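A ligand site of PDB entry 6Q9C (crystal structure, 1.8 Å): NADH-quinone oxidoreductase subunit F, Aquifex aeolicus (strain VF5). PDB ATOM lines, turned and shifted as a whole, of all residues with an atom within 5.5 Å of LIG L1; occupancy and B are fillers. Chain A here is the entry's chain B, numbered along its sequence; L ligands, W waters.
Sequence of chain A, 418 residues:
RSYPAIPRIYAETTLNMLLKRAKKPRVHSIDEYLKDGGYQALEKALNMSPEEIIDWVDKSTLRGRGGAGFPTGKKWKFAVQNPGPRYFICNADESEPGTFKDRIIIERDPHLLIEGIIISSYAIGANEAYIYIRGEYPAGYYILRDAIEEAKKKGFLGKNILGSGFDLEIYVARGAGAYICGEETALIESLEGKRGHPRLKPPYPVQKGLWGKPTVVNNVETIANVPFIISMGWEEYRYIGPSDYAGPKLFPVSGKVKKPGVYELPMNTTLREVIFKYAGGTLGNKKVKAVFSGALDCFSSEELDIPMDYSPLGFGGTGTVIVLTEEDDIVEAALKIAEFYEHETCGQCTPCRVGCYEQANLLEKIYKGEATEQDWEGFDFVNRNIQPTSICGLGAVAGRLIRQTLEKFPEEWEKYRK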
ATOM      1  N   ARG A  63      24.052   6.194 -20.931  1.00  0.00           N
ATOM      2  CA  ARG A  63      25.302   6.021 -20.155  1.00  0.00           C
ATOM      3  C   ARG A  63      25.221   4.678 -19.428  1.00  0.00           C
ATOM      4  O   ARG A  63      24.105   4.281 -19.050  1.00  0.00           O
ATOM      5  CB  ARG A  63      25.472   7.171 -19.158  1.00  0.00           C
ATOM      6  CG  ARG A  63      26.074   8.433 -19.769  1.00  0.00           C
ATOM      7  CD  ARG A  63      26.263   9.532 -18.748  1.00  0.00           C
ATOM      8  NE  ARG A  63      26.890  10.708 -19.356  1.00  0.00           N
ATOM      9  CZ  ARG A  63      28.193  10.927 -19.429  1.00  0.00           C
ATOM     10  NH1 ARG A  63      28.640  12.035 -20.008  1.00  0.00           N
ATOM     11  NH2 ARG A  63      29.069  10.060 -18.944  1.00  0.00           N
ATOM     12  N   GLY A  64      26.374   4.049 -19.232  1.00  0.00           N
ATOM     13  CA  GLY A  64      26.492   2.724 -18.589  1.00  0.00           C
ATOM     14  C   GLY A  64      25.731   2.657 -17.280  1.00  0.00           C
ATOM     15  O   GLY A  64      26.151   3.314 -16.291  1.00  0.00           O
ATOM     16  N   ARG A  65      24.692   1.832 -17.243  1.00  0.00           N
ATOM     17  CA  ARG A  65      23.805   1.619 -16.072  1.00  0.00           C
ATOM     18  C   ARG A  65      24.429   0.609 -15.105  1.00  0.00           C
ATOM     19  O   ARG A  65      23.824   0.361 -14.048  1.00  0.00           O
ATOM     20  CB  ARG A  65      22.436   1.138 -16.570  1.00  0.00           C
ATOM     21  CG  ARG A  65      21.767   2.081 -17.544  1.00  0.00           C
ATOM     22  CD  ARG A  65      21.453   3.422 -16.918  1.00  0.00           C
ATOM     23  NE  ARG A  65      20.375   4.129 -17.600  1.00  0.00           N
ATOM     24  CZ  ARG A  65      20.479   5.260 -18.286  1.00  0.00           C
ATOM     25  NH1 ARG A  65      19.392   5.797 -18.819  1.00  0.00           N
ATOM     26  NH2 ARG A  65      21.651   5.865 -18.450  1.00  0.00           N
ATOM     27  N   GLY A  66      25.586   0.051 -15.432  1.00  0.00           N
ATOM     28  CA  GLY A  66      26.313  -0.870 -14.541  1.00  0.00           C
ATOM     29  C   GLY A  66      26.874  -0.142 -13.329  1.00  0.00           C
ATOM     30  O   GLY A  66      27.185  -0.832 -12.337  1.00  0.00           O
ATOM     31  N   GLY A  67      27.024   1.189 -13.411  1.00  0.00           N
ATOM     32  CA  GLY A  67      27.431   2.013 -12.255  1.00  0.00           C
ATOM     33  C   GLY A  67      28.467   3.069 -12.589  1.00  0.00           C
ATOM     34  O   GLY A  67      28.532   4.052 -11.838  1.00  0.00           O
ATOM     35  N   ALA A  68      29.238   2.918 -13.671  1.00  0.00           N
ATOM     36  CA  ALA A  68      30.338   3.855 -14.021  1.00  0.00           C
ATOM     37  C   ALA A  68      29.832   4.971 -14.940  1.00  0.00           C
ATOM     38  O   ALA A  68      30.505   6.020 -15.000  1.00  0.00           O
ATOM     39  CB  ALA A  68      31.478   3.112 -14.654  1.00  0.00           C
ATOM     40  N   GLY A  69      28.707   4.766 -15.640  1.00  0.00           N
ATOM     41  CA  GLY A  69      28.083   5.791 -16.499  1.00  0.00           C
ATOM     42  C   GLY A  69      28.932   6.180 -17.705  1.00  0.00           C
ATOM     43  O   GLY A  69      28.783   7.324 -18.170  1.00  0.00           O
ATOM     44  N   PHE A  70      29.741   5.265 -18.248  1.00  0.00           N
ATOM     45  CA  PHE A  70      30.473   5.504 -19.509  1.00  0.00           C
ATOM     46  C   PHE A  70      29.472   5.648 -20.659  1.00  0.00           C
ATOM     47  O   PHE A  70      28.520   4.872 -20.747  1.00  0.00           O
ATOM     48  CB  PHE A  70      31.483   4.394 -19.813  1.00  0.00           C
ATOM     49  CG  PHE A  70      32.475   4.763 -20.868  1.00  0.00           C
ATOM     50  CD1 PHE A  70      33.656   5.422 -20.542  1.00  0.00           C
ATOM     51  CD2 PHE A  70      32.228   4.493 -22.209  1.00  0.00           C
ATOM     52  CE1 PHE A  70      34.563   5.771 -21.524  1.00  0.00           C
ATOM     53  CE2 PHE A  70      33.146   4.851 -23.190  1.00  0.00           C
ATOM     54  CZ  PHE A  70      34.315   5.487 -22.840  1.00  0.00           C
ATOM     55  N   THR A  72      27.562   4.969 -23.796  1.00  0.00           N
ATOM     56  CA  THR A  72      27.408   3.641 -24.442  1.00  0.00           C
ATOM     57  C   THR A  72      27.790   3.739 -25.931  1.00  0.00           C
ATOM     58  O   THR A  72      28.579   2.889 -26.389  1.00  0.00           O
ATOM     59  CB  THR A  72      25.988   3.118 -24.243  1.00  0.00           C
ATOM     60  OG1 THR A  72      25.720   3.198 -22.843  1.00  0.00           O
ATOM     61  CG2 THR A  72      25.808   1.695 -24.737  1.00  0.00           C
ATOM     62  N   LYS A  75      31.451   3.871 -26.430  1.00  0.00           N
ATOM     63  CA  LYS A  75      32.061   2.548 -26.166  1.00  0.00           C
ATOM     64  C   LYS A  75      31.961   1.696 -27.439  1.00  0.00           C
ATOM     65  O   LYS A  75      32.966   1.076 -27.828  1.00  0.00           O
ATOM     66  CB  LYS A  75      31.400   1.831 -24.975  1.00  0.00           C
ATOM     67  CG  LYS A  75      32.110   0.568 -24.523  1.00  0.00           C
ATOM     68  CD  LYS A  75      31.326  -0.257 -23.526  1.00  0.00           C
ATOM     69  CE  LYS A  75      31.149   0.429 -22.187  1.00  0.00           C
ATOM     70  NZ  LYS A  75      30.703  -0.504 -21.136  1.00  0.00           N
ATOM     71  N   ASN A  91      26.486  -8.105 -19.186  1.00  0.00           N
ATOM     72  CA  ASN A  91      26.899  -8.284 -17.775  1.00  0.00           C
ATOM     73  C   ASN A  91      25.642  -8.402 -16.901  1.00  0.00           C
ATOM     74  O   ASN A  91      25.019  -7.354 -16.628  1.00  0.00           O
ATOM     75  CB  ASN A  91      27.801  -7.139 -17.317  1.00  0.00           C
ATOM     76  CG  ASN A  91      28.541  -7.458 -16.038  1.00  0.00           C
ATOM     77  OD1 ASN A  91      28.092  -8.298 -15.251  1.00  0.00           O
ATOM     78  ND2 ASN A  91      29.665  -6.803 -15.811  1.00  0.00           N
ATOM     79  N   ALA A  92      25.297  -9.619 -16.483  1.00  0.00           N
ATOM     80  CA  ALA A  92      24.178  -9.936 -15.560  1.00  0.00           C
ATOM     81  C   ALA A  92      24.760 -10.503 -14.255  1.00  0.00           C
ATOM     82  O   ALA A  92      24.122 -11.356 -13.617  1.00  0.00           O
ATOM     83  CB  ALA A  92      23.217 -10.898 -16.209  1.00  0.00           C
ATOM     84  N   ASP A  93      25.946 -10.043 -13.844  1.00  0.00           N
ATOM     85  CA  ASP A  93      26.571 -10.573 -12.612  1.00  0.00           C
ATOM     86  C   ASP A  93      26.005  -9.893 -11.356  1.00  0.00           C
ATOM     87  O   ASP A  93      26.254 -10.434 -10.266  1.00  0.00           O
ATOM     88  CB  ASP A  93      28.092 -10.450 -12.626  1.00  0.00           C
ATOM     89  CG  ASP A  93      28.717 -11.421 -11.626  1.00  0.00           C
ATOM     90  OD1 ASP A  93      28.499 -12.636 -11.807  1.00  0.00           O
ATOM     91  OD2 ASP A  93      29.358 -10.941 -10.652  1.00  0.00           O
ATOM     92  N   GLU A  94      25.323  -8.749 -11.504  1.00  0.00           N
ATOM     93  CA  GLU A  94      24.714  -7.918 -10.433  1.00  0.00           C
ATOM     94  C   GLU A  94      24.940  -8.495  -9.029  1.00  0.00           C
ATOM     95  O   GLU A  94      24.124  -9.312  -8.583  1.00  0.00           O
ATOM     96  CB  GLU A  94      23.207  -7.781 -10.672  1.00  0.00           C
ATOM     97  CG  GLU A  94      22.492  -6.977  -9.613  1.00  0.00           C
ATOM     98  CD  GLU A  94      21.086  -6.608 -10.029  1.00  0.00           C
ATOM     99  OE1 GLU A  94      20.241  -7.526 -10.110  1.00  0.00           O
ATOM    100  OE2 GLU A  94      20.862  -5.416 -10.304  1.00  0.00           O
ATOM    101  N   SER A  95      26.011  -8.086  -8.347  1.00  0.00           N
ATOM    102  CA  SER A  95      26.371  -8.582  -6.993  1.00  0.00           C
ATOM    103  C   SER A  95      26.728  -7.442  -6.031  1.00  0.00           C
ATOM    104  O   SER A  95      27.102  -7.774  -4.891  1.00  0.00           O
ATOM    105  CB  SER A  95      27.476  -9.596  -7.088  1.00  0.00           C
ATOM    106  OG  SER A  95      27.055 -10.742  -7.816  1.00  0.00           O
ATOM    107  N   GLU A  96      26.575  -6.174  -6.414  1.00  0.00           N
ATOM    108  CA  GLU A  96      26.765  -5.014  -5.490  1.00  0.00           C
ATOM    109  C   GLU A  96      25.732  -5.110  -4.367  1.00  0.00           C
ATOM    110  O   GLU A  96      24.549  -5.285  -4.630  1.00  0.00           O
ATOM    111  CB  GLU A  96      26.611  -3.685  -6.226  1.00  0.00           C
ATOM    112  CG  GLU A  96      26.957  -2.467  -5.382  1.00  0.00           C
ATOM    113  CD  GLU A  96      28.438  -2.247  -5.151  1.00  0.00           C
ATOM    114  OE1 GLU A  96      29.241  -3.174  -5.446  1.00  0.00           O
ATOM    115  OE2 GLU A  96      28.794  -1.149  -4.668  1.00  0.00           O
ATOM    116  N   ASP A 102      18.699  -5.275 -12.028  1.00  0.00           N
ATOM    117  CA  ASP A 102      18.881  -6.058 -13.291  1.00  0.00           C
ATOM    118  C   ASP A 102      18.009  -7.326 -13.286  1.00  0.00           C
ATOM    119  O   ASP A 102      17.492  -7.694 -14.358  1.00  0.00           O
ATOM    120  CB  ASP A 102      20.345  -6.445 -13.516  1.00  0.00           C
ATOM    121  CG  ASP A 102      21.267  -5.262 -13.710  1.00  0.00           C
ATOM    122  OD1 ASP A 102      20.769  -4.154 -13.965  1.00  0.00           O
ATOM    123  OD2 ASP A 102      22.494  -5.460 -13.617  1.00  0.00           O
ATOM    124  N   TYR A 179      31.986 -12.000  -6.690  1.00  0.00           N
ATOM    125  CA  TYR A 179      31.633 -10.582  -6.984  1.00  0.00           C
ATOM    126  C   TYR A 179      32.567 -10.007  -8.047  1.00  0.00           C
ATOM    127  O   TYR A 179      32.113  -9.225  -8.888  1.00  0.00           O
ATOM    128  CB  TYR A 179      31.712  -9.774  -5.694  1.00  0.00           C
ATOM    129  CG  TYR A 179      31.719  -8.277  -5.793  1.00  0.00           C
ATOM    130  CD1 TYR A 179      30.560  -7.549  -6.011  1.00  0.00           C
ATOM    131  CD2 TYR A 179      32.881  -7.572  -5.546  1.00  0.00           C
ATOM    132  CE1 TYR A 179      30.575  -6.166  -6.017  1.00  0.00           C
ATOM    133  CE2 TYR A 179      32.907  -6.180  -5.550  1.00  0.00           C
ATOM    134  CZ  TYR A 179      31.752  -5.476  -5.781  1.00  0.00           C
ATOM    135  OH  TYR A 179      31.796  -4.112  -5.758  1.00  0.00           O
ATOM    136  N   ILE A 180      33.852 -10.369  -7.992  1.00  0.00           N
ATOM    137  CA  ILE A 180      34.898  -9.808  -8.907  1.00  0.00           C
ATOM    138  C   ILE A 180      34.579 -10.207 -10.360  1.00  0.00           C
ATOM    139  O   ILE A 180      35.048  -9.499 -11.243  1.00  0.00           O
ATOM    140  CB  ILE A 180      36.313 -10.236  -8.469  1.00  0.00           C
ATOM    141  CG1 ILE A 180      37.392  -9.396  -9.154  1.00  0.00           C
ATOM    142  CG2 ILE A 180      36.543 -11.718  -8.706  1.00  0.00           C
ATOM    143  CD1 ILE A 180      37.185  -7.906  -9.000  1.00  0.00           C
ATOM    144  N   GLY A 182      31.960  -9.790 -11.956  1.00  0.00           N
ATOM    145  CA  GLY A 182      31.229  -8.648 -12.536  1.00  0.00           C
ATOM    146  C   GLY A 182      32.164  -7.615 -13.125  1.00  0.00           C
ATOM    147  O   GLY A 182      31.728  -6.851 -13.987  1.00  0.00           O
ATOM    148  N   GLU A 183      33.417  -7.549 -12.656  1.00  0.00           N
ATOM    149  CA  GLU A 183      34.422  -6.662 -13.285  1.00  0.00           C
ATOM    150  C   GLU A 183      34.626  -7.175 -14.711  1.00  0.00           C
ATOM    151  O   GLU A 183      34.835  -8.398 -14.879  1.00  0.00           O
ATOM    152  CB  GLU A 183      35.702  -6.625 -12.439  1.00  0.00           C
ATOM    153  CG  GLU A 183      36.599  -5.428 -12.725  1.00  0.00           C
ATOM    154  CD  GLU A 183      37.514  -5.543 -13.940  1.00  0.00           C
ATOM    155  OE1 GLU A 183      37.596  -6.636 -14.567  1.00  0.00           O
ATOM    156  OE2 GLU A 183      38.166  -4.528 -14.243  1.00  0.00           O
ATOM    157  N   GLU A 184      34.503  -6.300 -15.709  1.00  0.00           N
ATOM    158  CA  GLU A 184      34.333  -6.717 -17.131  1.00  0.00           C
ATOM    159  C   GLU A 184      35.487  -7.618 -17.588  1.00  0.00           C
ATOM    160  O   GLU A 184      35.208  -8.549 -18.361  1.00  0.00           O
ATOM    161  CB  GLU A 184      34.173  -5.505 -18.058  1.00  0.00           C
ATOM    162  CG  GLU A 184      35.339  -4.536 -18.012  1.00  0.00           C
ATOM    163  CD  GLU A 184      35.243  -3.363 -18.968  1.00  0.00           C
ATOM    164  OE1 GLU A 184      34.235  -3.288 -19.719  1.00  0.00           O
ATOM    165  OE2 GLU A 184      36.180  -2.532 -18.969  1.00  0.00           O
ATOM    166  N   VAL A 217      31.376  -4.954 -23.381  1.00  0.00           N
ATOM    167  CA  VAL A 217      30.635  -5.377 -22.156  1.00  0.00           C
ATOM    168  C   VAL A 217      29.671  -4.253 -21.805  1.00  0.00           C
ATOM    169  O   VAL A 217      30.125  -3.103 -21.602  1.00  0.00           O
ATOM    170  CB  VAL A 217      31.567  -5.711 -20.976  1.00  0.00           C
ATOM    171  CG1 VAL A 217      30.764  -6.213 -19.773  1.00  0.00           C
ATOM    172  CG2 VAL A 217      32.637  -6.710 -21.379  1.00  0.00           C
ATOM    173  N   ASN A 218      28.390  -4.578 -21.725  1.00  0.00           N
ATOM    174  CA  ASN A 218      27.345  -3.646 -21.236  1.00  0.00           C
ATOM    175  C   ASN A 218      26.487  -4.344 -20.195  1.00  0.00           C
ATOM    176  O   ASN A 218      26.299  -5.581 -20.268  1.00  0.00           O
ATOM    177  CB  ASN A 218      26.486  -3.084 -22.368  1.00  0.00           C
ATOM    178  CG  ASN A 218      27.114  -1.876 -23.053  1.00  0.00           C
ATOM    179  OD1 ASN A 218      27.236  -1.866 -24.269  1.00  0.00           O
ATOM    180  ND2 ASN A 218      27.480  -0.874 -22.269  1.00  0.00           N
ATOM    181  N   ASN A 219      25.980  -3.547 -19.275  1.00  0.00           N
ATOM    182  CA  ASN A 219      25.102  -3.963 -18.162  1.00  0.00           C
ATOM    183  C   ASN A 219      23.708  -4.289 -18.728  1.00  0.00           C
ATOM    184  O   ASN A 219      23.305  -3.646 -19.719  1.00  0.00           O
ATOM    185  CB  ASN A 219      25.078  -2.870 -17.100  1.00  0.00           C
ATOM    186  CG  ASN A 219      24.026  -3.101 -16.032  1.00  0.00           C
ATOM    187  OD1 ASN A 219      22.966  -2.507 -16.092  1.00  0.00           O
ATOM    188  ND2 ASN A 219      24.323  -3.978 -15.089  1.00  0.00           N
ATOM    189  N   VAL A 220      23.012  -5.228 -18.097  1.00  0.00           N
ATOM    190  CA  VAL A 220      21.598  -5.610 -18.386  1.00  0.00           C
ATOM    191  C   VAL A 220      20.745  -4.354 -18.625  1.00  0.00           C
ATOM    192  O   VAL A 220      20.066  -4.272 -19.674  1.00  0.00           O
ATOM    193  CB  VAL A 220      21.022  -6.466 -17.243  1.00  0.00           C
ATOM    194  CG1 VAL A 220      19.509  -6.601 -17.356  1.00  0.00           C
ATOM    195  CG2 VAL A 220      21.676  -7.833 -17.171  1.00  0.00           C
ATOM    196  N   THR A 222      21.538  -1.118 -19.175  1.00  0.00           N
ATOM    197  CA  THR A 222      22.010  -0.361 -20.373  1.00  0.00           C
ATOM    198  C   THR A 222      21.362  -0.951 -21.639  1.00  0.00           C
ATOM    199  O   THR A 222      20.735  -0.195 -22.406  1.00  0.00           O
ATOM    200  CB  THR A 222      23.536  -0.392 -20.505  1.00  0.00           C
ATOM    201  OG1 THR A 222      24.082  -0.142 -19.208  1.00  0.00           O
ATOM    202  CG2 THR A 222      24.051   0.626 -21.499  1.00  0.00           C
ATOM    203  N   CYS A 392      42.100  -3.013 -10.662  1.00  0.00           N
ATOM    204  CA  CYS A 392      40.632  -2.935 -10.901  1.00  0.00           C
ATOM    205  C   CYS A 392      39.948  -2.056  -9.853  1.00  0.00           C
ATOM    206  O   CYS A 392      40.600  -1.669  -8.869  1.00  0.00           O
ATOM    207  CB  CYS A 392      40.007  -4.327 -11.019  1.00  0.00           C
ATOM    208  SG  CYS A 392      39.290  -4.986  -9.500  1.00  0.00           S
ATOM    209  N   GLY A 393      38.696  -1.719 -10.121  1.00  0.00           N
ATOM    210  CA  GLY A 393      37.862  -0.808  -9.308  1.00  0.00           C
ATOM    211  C   GLY A 393      37.660  -1.272  -7.871  1.00  0.00           C
ATOM    212  O   GLY A 393      37.329  -0.403  -7.050  1.00  0.00           O
ATOM    213  N   LEU A 394      37.811  -2.570  -7.570  1.00  0.00           N
ATOM    214  CA  LEU A 394      37.568  -3.108  -6.205  1.00  0.00           C
ATOM    215  C   LEU A 394      38.605  -2.502  -5.249  1.00  0.00           C
ATOM    216  O   LEU A 394      38.203  -1.853  -4.266  1.00  0.00           O
ATOM    217  CB  LEU A 394      37.613  -4.643  -6.185  1.00  0.00           C
ATOM    218  CG  LEU A 394      37.043  -5.293  -4.912  1.00  0.00           C
ATOM    219  CD1 LEU A 394      36.426  -6.655  -5.204  1.00  0.00           C
ATOM    220  CD2 LEU A 394      38.106  -5.423  -3.833  1.00  0.00           C
HETATM  221  N1  LIG L   1      28.970  -4.140 -14.031  1.00  0.00           N
HETATM  222  C1  LIG L   1      27.804  -4.823 -14.187  1.00  0.00           C
HETATM  223  O1  LIG L   1      27.056  -4.626 -15.153  1.00  0.00           O
HETATM  224  N2  LIG L   1      27.466  -5.818 -13.276  1.00  0.00           N
HETATM  225  C2  LIG L   1      28.239  -6.233 -12.199  1.00  0.00           C
HETATM  226  O2  LIG L   1      27.829  -7.105 -11.433  1.00  0.00           O
HETATM  227  C3  LIG L   1      29.508  -5.524 -12.079  1.00  0.00           C
HETATM  228  N3  LIG L   1      30.325  -5.882 -11.125  1.00  0.00           N
HETATM  229  C4  LIG L   1      31.536  -5.210 -11.027  1.00  0.00           C
HETATM  230  C5  LIG L   1      32.433  -5.576 -10.006  1.00  0.00           C
HETATM  231  C6  LIG L   1      33.633  -4.893  -9.826  1.00  0.00           C
HETATM  232  C7  LIG L   1      34.544  -5.296  -8.688  1.00  0.00           C
HETATM  233  C8  LIG L   1      33.954  -3.830 -10.686  1.00  0.00           C
HETATM  234  C9  LIG L   1      35.211  -3.017 -10.490  1.00  0.00           C
HETATM  235  C10 LIG L   1      33.090  -3.481 -11.711  1.00  0.00           C
HETATM  236  C11 LIG L   1      31.879  -4.151 -11.888  1.00  0.00           C
HETATM  237  N4  LIG L   1      30.960  -3.803 -12.911  1.00  0.00           N
HETATM  238  C12 LIG L   1      29.771  -4.475 -13.035  1.00  0.00           C
HETATM  239  C13 LIG L   1      31.286  -2.788 -13.922  1.00  0.00           C
HETATM  240  C14 LIG L   1      31.841  -3.407 -15.190  1.00  0.00           C
HETATM  241  O3  LIG L   1      33.254  -3.610 -15.079  1.00  0.00           O
HETATM  242  C15 LIG L   1      31.551  -2.547 -16.416  1.00  0.00           C
HETATM  243  O4  LIG L   1      31.896  -1.182 -16.176  1.00  0.00           O
HETATM  244  C16 LIG L   1      30.104  -2.565 -16.908  1.00  0.00           C
HETATM  245  O5  LIG L   1      29.597  -3.892 -16.932  1.00  0.00           O
HETATM  246  C17 LIG L   1      30.033  -1.924 -18.282  1.00  0.00           C
HETATM  247  O6  LIG L   1      28.648  -1.839 -18.692  1.00  0.00           O
HETATM  248  P1  LIG L   1      27.911  -0.425 -18.711  1.00  0.00           P
HETATM  249  O7  LIG L   1      27.628   0.065 -17.308  1.00  0.00           O
HETATM  250  O8  LIG L   1      28.793   0.534 -19.476  1.00  0.00           O
HETATM  251  O9  LIG L   1      26.622  -0.692 -19.522  1.00  0.00           O
HETATM  252  P1  LG2 L   2      35.321   2.382 -15.532  1.00  0.00           P
HETATM  253  O1  LG2 L   2      34.859   3.782 -15.327  1.00  0.00           O
HETATM  254  O2  LG2 L   2      36.825   2.164 -15.459  1.00  0.00           O
HETATM  255  O3  LG2 L   2      34.831   1.817 -16.968  1.00  0.00           O
HETATM  256  C1  LG2 L   2      33.432   1.851 -17.300  1.00  0.00           C
HETATM  257  C2  LG2 L   2      33.221   1.274 -18.679  1.00  0.00           C
HETATM  258  O4  LG2 L   2      33.749   2.186 -19.669  1.00  0.00           O
HETATM  259  C3  LG2 L   2      33.924  -0.064 -18.932  1.00  0.00           C
HETATM  260  O5  LG2 L   2      33.144  -0.888 -19.787  1.00  0.00           O
HETATM  261  C4  LG2 L   2      35.239   0.359 -19.576  1.00  0.00           C
HETATM  262  O6  LG2 L   2      35.771  -0.637 -20.436  1.00  0.00           O
HETATM  263  C5  LG2 L   2      34.797   1.571 -20.400  1.00  0.00           C
HETATM  264  N1  LG2 L   2      35.859   2.551 -20.599  1.00  0.00           N
HETATM  265  C6  LG2 L   2      36.398   3.396 -19.655  1.00  0.00           C
HETATM  266  N2  LG2 L   2      37.402   4.119 -20.099  1.00  0.00           N
HETATM  267  C7  LG2 L   2      37.539   3.725 -21.421  1.00  0.00           C
HETATM  268  C8  LG2 L   2      38.439   4.099 -22.435  1.00  0.00           C
HETATM  269  N3  LG2 L   2      39.444   4.962 -22.252  1.00  0.00           N
HETATM  270  N4  LG2 L   2      38.292   3.518 -23.653  1.00  0.00           N
HETATM  271  C9  LG2 L   2      37.310   2.625 -23.818  1.00  0.00           C
HETATM  272  N5  LG2 L   2      36.417   2.186 -22.937  1.00  0.00           N
HETATM  273  C10 LG2 L   2      36.585   2.767 -21.744  1.00  0.00           C
HETATM  274  O7  LG2 L   2      34.637   1.433 -14.458  1.00  0.00           O
HETATM  275  P2  LG2 L   2      34.651  -0.090 -14.018  1.00  0.00           P
HETATM  276  O8  LG2 L   2      35.882  -0.300 -13.150  1.00  0.00           O
HETATM  277  O9  LG2 L   2      34.490  -1.025 -15.157  1.00  0.00           O
HETATM  278  O10 LG2 L   2      33.363  -0.166 -13.035  1.00  0.00           O
HETATM  279  C11 LG2 L   2      33.209   0.527 -11.779  1.00  0.00           C
HETATM  280  C12 LG2 L   2      31.751   0.546 -11.393  1.00  0.00           C
HETATM  281  O11 LG2 L   2      31.257  -0.798 -11.217  1.00  0.00           O
HETATM  282  C13 LG2 L   2      31.430   1.252 -10.071  1.00  0.00           C
HETATM  283  O12 LG2 L   2      31.083   2.609 -10.310  1.00  0.00           O
HETATM  284  C14 LG2 L   2      30.255   0.445  -9.489  1.00  0.00           C
HETATM  285  O13 LG2 L   2      29.083   1.250  -9.401  1.00  0.00           O
HETATM  286  C15 LG2 L   2      30.038  -0.674 -10.525  1.00  0.00           C
HETATM  287  N6  LG2 L   2      29.668  -1.954  -9.953  1.00  0.00           N
HETATM  288  C16 LG2 L   2      28.385  -2.529 -10.176  1.00  0.00           C
HETATM  289  C17 LG2 L   2      28.011  -3.716  -9.656  1.00  0.00           C
HETATM  290  C18 LG2 L   2      26.648  -4.201  -9.905  1.00  0.00           C
HETATM  291  O14 LG2 L   2      26.196  -5.123  -9.206  1.00  0.00           O
HETATM  292  N7  LG2 L   2      25.938  -3.624 -10.872  1.00  0.00           N
HETATM  293  C19 LG2 L   2      28.938  -4.504  -8.807  1.00  0.00           C
HETATM  294  C20 LG2 L   2      30.250  -3.822  -8.639  1.00  0.00           C
HETATM  295  C21 LG2 L   2      30.544  -2.646  -9.175  1.00  0.00           C
HETATM  296  O   HOH W   1      29.466  -8.457  -9.564  1.00  0.00           O
HETATM  297  O   HOH W   2      29.553   0.598 -15.548  1.00  0.00           O
HETATM  298  O   HOH W   3      28.012   2.159 -21.508  1.00  0.00           O
HETATM  299  O   HOH W   4      29.922   2.390 -17.763  1.00  0.00           O
HETATM  300  O   HOH W   5      24.712  -6.948 -13.813  1.00  0.00           O
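The side-chain hydroxyl of Thr 222 lies within hydrogen-bond range of an oxygen (O9) of LIG L1 (2.6 Å). O8 of LIG L1 lies within salt-bridge range of NZ of Lys 75, at 2.7 Å. N of Gly 66 is in hydrogen-bond range of O7 of LIG L1, at 2.8 Å. An oxygen (O9) of LIG L1 is in hydrogen-bond range of the backbone NH (N) of Asn 219, 2.9 Å away. ND2 of Asn 219 lies within hydrogen-bond range of O1 of LIG L1, at 2.8 Å. ND2 of Asn 218 lies within hydrogen-bond range of O9 of LIG L1, at 2.9 Å. N of Glu 94 sits at hydrogen-bond distance from O2 of LIG L1. The backbone NH of Glu 184 lies within hydrogen-bond range of an oxygen (O3) of LIG L1. ND2 of Asn 91 is in hydrogen-bond range of O5 of LIG L1, at 3.1 Å. The backbone NH of Arg 65 lies within hydrogen-bond range of an oxygen (O7) of LIG L1. An oxygen (O5) of LG2 L2 lies within hydrogen-bond range of the side-chain amino group of Lys 75, 2.8 Å away. O of Gly 66 sits close to N7 of LG2 L2 (3.4 Å). OE2 of Glu 184 sits at hydrogen-bond distance from O6 of LG2 L2 (2.4 Å). The backbone NH (N) of Ser 95 lies within hydrogen-bond range of an oxygen (O14) of LG2 L2, at 3.1 Å. The backbone carbonyl oxygen (O) of Gly 67 sits at hydrogen-bond distance from an oxygen (O12) of LG2 L2, at 3.3 Å. N of Glu 96 lies within hydrogen-bond range of O14 of LG2 L2.
An oxygen (O9) of LG2 L2 is in hydrogen-bond range of an oxygen (O4) of LIG L1 (2.8 Å).
The side-chain amino group (NZ) of Lys 75 sits close to the side-chain amide nitrogen (ND2) of Asn 218, 3.4 Å away. The side-chain amino group of Lys 75 is in hydrogen-bond range of the backbone carbonyl oxygen of Val 217. ND2 of Asn 219 lies within hydrogen-bond range of OD2 of Asp 102. The backbone NH (N) of Asn 91 sits at hydrogen-bond distance from the backbone carbonyl oxygen (O) of Asn 218 (2.8 Å). The backbone NH (N) of Asp 102 sits at hydrogen-bond distance from the side-chain carboxylate (OE2) of Glu 94. The side-chain amide oxygen (OD1) of Asn 91 lies within hydrogen-bond range of the backbone NH (N) of Asp 93 (3.1 Å). The backbone NH (N) of Gly 182 is in hydrogen-bond range of the side-chain carboxylate (OD2) of Asp 93, 3.1 Å away. OE1 of Glu 96 is in hydrogen-bond range of OH of Tyr 179 (2.7 Å).
N4 of LIG L1 sits close to O of Gly 182 (3.3 Å). An oxygen (O6) of LIG L1 sits close to the backbone carbonyl oxygen (O) of Val 217, 3.5 Å away. Residues that only touch LIG L1: Gly 64 (3.2 Å), Asp 93 (3.3 Å), Ser 95 (3.7 Å), Tyr 179 (3.6 Å), Ile 180 (3.7 Å), Glu 183 (3.4 Å), Gly 393 (3.6 Å) and Leu 394 (3.9 Å). Hydrophobic or aromatic side chains within 4 Å of LIG L1: Tyr 179, Ile 180 and Val 217. Of the 30 residues printed, 19 come within 4 Å of LIG L1.
Water W2 lies within hydrogen-bond range of an oxygen (O7) of LIG L1 (2.7 Å), the backbone NH (N) of Ala 68 (3.0 Å) and the backbone NH (N) of Gly 67 (3.4 Å). Water W3 lies within hydrogen-bond range of O8 of LIG L1 (2.7 Å), OG1 of Thr 72 (2.8 Å), O of Phe 70 (2.9 Å), ND2 of Asn 218 (3.2 Å) and N of Gly 64 (3.4 Å). Water W4 lies within hydrogen-bond range of an oxygen (O8) of LIG L1 (2.8 Å), the backbone NH of Phe 70 (2.9 Å) and the backbone NH of Gly 69 (3.4 Å).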
